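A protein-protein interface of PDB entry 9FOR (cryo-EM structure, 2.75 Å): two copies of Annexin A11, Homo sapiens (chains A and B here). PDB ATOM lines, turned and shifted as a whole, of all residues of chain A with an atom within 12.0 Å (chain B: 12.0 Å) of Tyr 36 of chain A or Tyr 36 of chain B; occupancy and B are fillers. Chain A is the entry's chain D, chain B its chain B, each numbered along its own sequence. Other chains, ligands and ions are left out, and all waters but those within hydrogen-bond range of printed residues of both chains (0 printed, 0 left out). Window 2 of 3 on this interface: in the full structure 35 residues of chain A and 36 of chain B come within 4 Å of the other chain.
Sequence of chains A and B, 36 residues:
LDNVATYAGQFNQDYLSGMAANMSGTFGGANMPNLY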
ATOM      1  N   ASN A  31      16.530  16.771  -3.825  1.00  0.00           N
ATOM      2  CA  ASN A  31      16.163  17.830  -2.916  1.00  0.00           C
ATOM      3  C   ASN A  31      15.105  18.712  -3.571  1.00  0.00           C
ATOM      4  O   ASN A  31      15.105  18.799  -4.791  1.00  0.00           O
ATOM      5  CB  ASN A  31      17.454  18.554  -2.587  1.00  0.00           C
ATOM      6  CG  ASN A  31      18.467  17.578  -2.035  1.00  0.00           C
ATOM      7  OD1 ASN A  31      18.209  16.969  -0.997  1.00  0.00           O
ATOM      8  ND2 ASN A  31      19.586  17.362  -2.701  1.00  0.00           N
ATOM      9  N   MET A  32      14.220  19.347  -2.782  1.00  0.00           N
ATOM     10  CA  MET A  32      13.135  20.165  -3.312  1.00  0.00           C
ATOM     11  C   MET A  32      12.831  21.396  -2.450  1.00  0.00           C
ATOM     12  O   MET A  32      11.889  21.407  -1.673  1.00  0.00           O
ATOM     13  CB  MET A  32      11.832  19.366  -3.370  1.00  0.00           C
ATOM     14  CG  MET A  32      11.906  18.137  -4.229  1.00  0.00           C
ATOM     15  SD  MET A  32      10.300  17.314  -4.308  1.00  0.00           S
ATOM     16  CE  MET A  32       9.251  18.519  -5.136  1.00  0.00           C
ATOM     17  N   PRO A  33      13.578  22.508  -2.565  1.00  0.00           N
ATOM     18  CA  PRO A  33      13.130  23.774  -1.974  1.00  0.00           C
ATOM     19  C   PRO A  33      11.870  24.355  -2.604  1.00  0.00           C
ATOM     20  O   PRO A  33      11.873  24.549  -3.804  1.00  0.00           O
ATOM     21  CB  PRO A  33      14.315  24.716  -2.185  1.00  0.00           C
ATOM     22  CG  PRO A  33      15.221  24.038  -3.169  1.00  0.00           C
ATOM     23  CD  PRO A  33      14.908  22.566  -3.188  1.00  0.00           C
ATOM     24  N   ASN A  34      10.839  24.670  -1.807  1.00  0.00           N
ATOM     25  CA  ASN A  34       9.603  25.262  -2.301  1.00  0.00           C
ATOM     26  C   ASN A  34       9.285  26.578  -1.607  1.00  0.00           C
ATOM     27  O   ASN A  34       9.305  26.637  -0.381  1.00  0.00           O
ATOM     28  CB  ASN A  34       8.326  24.526  -1.914  1.00  0.00           C
ATOM     29  CG  ASN A  34       8.309  23.103  -2.385  1.00  0.00           C
ATOM     30  OD1 ASN A  34       7.813  22.812  -3.479  1.00  0.00           O
ATOM     31  ND2 ASN A  34       8.794  22.204  -1.545  1.00  0.00           N
ATOM     32  N   LEU A  35       8.835  27.558  -2.403  1.00  0.00           N
ATOM     33  CA  LEU A  35       8.334  28.828  -1.900  1.00  0.00           C
ATOM     34  C   LEU A  35       6.960  29.079  -2.496  1.00  0.00           C
ATOM     35  O   LEU A  35       6.875  29.352  -3.683  1.00  0.00           O
ATOM     36  CB  LEU A  35       9.346  29.895  -2.309  1.00  0.00           C
ATOM     37  CG  LEU A  35       8.848  31.345  -2.354  1.00  0.00           C
ATOM     38  CD1 LEU A  35       8.038  31.706  -1.153  1.00  0.00           C
ATOM     39  CD2 LEU A  35      10.020  32.303  -2.464  1.00  0.00           C
ATOM     40  N   TYR A  36       5.910  29.035  -1.672  1.00  0.00           N
ATOM     41  CA  TYR A  36       4.543  29.291  -2.128  1.00  0.00           C
ATOM     42  C   TYR A  36       4.232  30.802  -2.095  1.00  0.00           C
ATOM     43  O   TYR A  36       4.111  31.402  -0.995  1.00  0.00           O
ATOM     44  CB  TYR A  36       3.465  28.572  -1.312  1.00  0.00           C
ATOM     45  CG  TYR A  36       3.678  27.068  -1.195  1.00  0.00           C
ATOM     46  CD1 TYR A  36       2.998  26.185  -2.017  1.00  0.00           C
ATOM     47  CD2 TYR A  36       4.569  26.534  -0.268  1.00  0.00           C
ATOM     48  CE1 TYR A  36       3.196  24.816  -1.922  1.00  0.00           C
ATOM     49  CE2 TYR A  36       4.786  25.170  -0.169  1.00  0.00           C
ATOM     50  CZ  TYR A  36       4.095  24.305  -1.000  1.00  0.00           C
ATOM     51  OH  TYR A  36       4.302  22.956  -0.901  1.00  0.00           O
ATOM     52  N   ASN B  31      16.982  17.190  -8.812  1.00  0.00           N
ATOM     53  CA  ASN B  31      16.576  18.237  -7.905  1.00  0.00           C
ATOM     54  C   ASN B  31      15.495  19.085  -8.566  1.00  0.00           C
ATOM     55  O   ASN B  31      15.499  19.172  -9.786  1.00  0.00           O
ATOM     56  CB  ASN B  31      17.841  19.000  -7.568  1.00  0.00           C
ATOM     57  CG  ASN B  31      18.882  18.057  -7.010  1.00  0.00           C
ATOM     58  OD1 ASN B  31      18.638  17.439  -5.974  1.00  0.00           O
ATOM     59  ND2 ASN B  31      20.011  17.876  -7.670  1.00  0.00           N
ATOM     60  N   MET B  32      14.585  19.691  -7.782  1.00  0.00           N
ATOM     61  CA  MET B  32      13.478  20.475  -8.319  1.00  0.00           C
ATOM     62  C   MET B  32      13.131  21.696  -7.458  1.00  0.00           C
ATOM     63  O   MET B  32      12.185  21.677  -6.687  1.00  0.00           O
ATOM     64  CB  MET B  32      12.202  19.636  -8.384  1.00  0.00           C
ATOM     65  CG  MET B  32      12.318  18.410  -9.242  1.00  0.00           C
ATOM     66  SD  MET B  32      10.739  17.537  -9.330  1.00  0.00           S
ATOM     67  CE  MET B  32       9.658  18.708 -10.164  1.00  0.00           C
ATOM     68  N   PRO B  33      13.843  22.831  -7.569  1.00  0.00           N
ATOM     69  CA  PRO B  33      13.352  24.083  -6.980  1.00  0.00           C
ATOM     70  C   PRO B  33      12.079  24.623  -7.617  1.00  0.00           C
ATOM     71  O   PRO B  33      12.083  24.818  -8.818  1.00  0.00           O
ATOM     72  CB  PRO B  33      14.508  25.061  -7.184  1.00  0.00           C
ATOM     73  CG  PRO B  33      15.440  24.412  -8.163  1.00  0.00           C
ATOM     74  CD  PRO B  33      15.174  22.931  -8.184  1.00  0.00           C
ATOM     75  N   ASN B  34      11.034  24.906  -6.826  1.00  0.00           N
ATOM     76  CA  ASN B  34       9.783  25.459  -7.327  1.00  0.00           C
ATOM     77  C   ASN B  34       9.419  26.764  -6.635  1.00  0.00           C
ATOM     78  O   ASN B  34       9.430  26.823  -5.409  1.00  0.00           O
ATOM     79  CB  ASN B  34       8.526  24.683  -6.948  1.00  0.00           C
ATOM     80  CG  ASN B  34       8.558  23.261  -7.419  1.00  0.00           C
ATOM     81  OD1 ASN B  34       8.077  22.954  -8.515  1.00  0.00           O
ATOM     82  ND2 ASN B  34       9.066  22.378  -6.576  1.00  0.00           N
ATOM     83  N   LEU B  35       8.943  27.729  -7.433  1.00  0.00           N
ATOM     84  CA  LEU B  35       8.400  28.983  -6.934  1.00  0.00           C
ATOM     85  C   LEU B  35       7.022  29.192  -7.537  1.00  0.00           C
ATOM     86  O   LEU B  35       6.935  29.462  -8.725  1.00  0.00           O
ATOM     87  CB  LEU B  35       9.380  30.082  -7.337  1.00  0.00           C
ATOM     88  CG  LEU B  35       8.836  31.514  -7.384  1.00  0.00           C
ATOM     89  CD1 LEU B  35       8.009  31.850  -6.188  1.00  0.00           C
ATOM     90  CD2 LEU B  35       9.979  32.509  -7.488  1.00  0.00           C
ATOM     91  N   TYR B  36       5.969  29.114  -6.719  1.00  0.00           N
ATOM     92  CA  TYR B  36       4.597  29.327  -7.183  1.00  0.00           C
ATOM     93  C   TYR B  36       4.239  30.827  -7.151  1.00  0.00           C
ATOM     94  O   TYR B  36       4.094  31.423  -6.052  1.00  0.00           O
ATOM     95  CB  TYR B  36       3.538  28.573  -6.373  1.00  0.00           C
ATOM     96  CG  TYR B  36       3.798  27.078  -6.255  1.00  0.00           C
ATOM     97  CD1 TYR B  36       3.150  26.173  -7.081  1.00  0.00           C
ATOM     98  CD2 TYR B  36       4.699  26.571  -5.323  1.00  0.00           C
ATOM     99  CE1 TYR B  36       3.391  24.811  -6.985  1.00  0.00           C
ATOM    100  CE2 TYR B  36       4.958  25.215  -5.222  1.00  0.00           C
ATOM    101  CZ  TYR B  36       4.300  24.329  -6.057  1.00  0.00           C
ATOM    102  OH  TYR B  36       4.548  22.987  -5.958  1.00  0.00           O
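Of the 6 printed residues of chain A, 6 touch a printed residue of chain B. Hydrophobic or aromatic side chains of chain A that line the printed part of chain B: Leu 35 and Tyr 36. Hydrophobic or aromatic side chains of chain B within 4 Å of the printed part of chain A: Leu 35 and Tyr 36. Among the printed residues, 10 pairs touch across the chains.
O of Met 32 of chain B is in hydrogen-bond range of ND2 of Asn 34 of chain B (3.2 Å). The backbone carbonyl oxygen (O) of Met 32 of chain A sits at hydrogen-bond distance from the side-chain amide nitrogen (ND2) of Asn 34 of chain A (3.2 Å).
Of chain B, only Tyr 36 comes within 4 Å of Tyr 36 of chain A. Of chain A, only Leu 35 and Tyr 36 come within 4 Å of Tyr 36 of chain B. Of chain B, only Asn 34 (3.4 Å) comes within 4 Å of Asn 34 of chain A. Printed residues of chain A within 4 Å of Met 32 of chain B: Asn 31 (3.2 Å) and Met 32 (3.8 Å). Printed residues of chain B within 4 Å of Asn 31 of chain A: Asn 31 (3.1 Å) and Met 32 (3.2 Å). The nearest printed residue of chain B that does not touch Met 32 of chain A is Asn 34 of chain B (4.1 Å).
Among the printed residues, pairs that only touch across the chains: Met 32 of chain A with Met 32 of chain B (3.8 Å), Pro 33 of chain A with Pro 33 of chain B (3.5 Å), Leu 35 of chain A with Leu 35 of chain B (3.6 Å) and Tyr 36 of chain A with Tyr 36 of chain B (3.7 Å).
The backbone NH of Asn 31 of chain A sits at hydrogen-bond distance from the side-chain amide oxygen of Asn 31 of chain B, 3.1 Å away. N of Met 32 of chain B lies within hydrogen-bond range of O of Asn 31 of chain A, at 3.2 Å. N of Asn 34 of chain B sits at hydrogen-bond distance from O of Pro 33 of chain A. The side-chain amide oxygen of Asn 34 of chain A lies within hydrogen-bond range of the side-chain amide nitrogen of Asn 34 of chain B (3.4 Å). N of Leu 35 of chain A is in hydrogen-bond range of O of Asn 34 of chain B, at 3.2 Å. O of Leu 35 of chain A lies within hydrogen-bond range of N of Tyr 36 of chain B.
Asn 31 of chain A touches Met 32 of chain B, but with the chains exchanged Met 32 of chain A does not touch Asn 31 of chain B (5.7 Å). Pro 33 of chain B touches its own counterpart, Pro 33 of chain A. Pro 33 of chain A touches Asn 34 of chain B, but with the chains exchanged Asn 34 of chain A does not touch Pro 33 of chain B (5.8 Å). Leu 35 of chain B touches its own counterpart, Leu 35 of chain A. Positions printed for both chains: 31, 32, 33, 34, 35 and 36. Of the 10 pairs that touch across the chains among the printed residues, 6 have their exchanged pair printed and touching as well.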
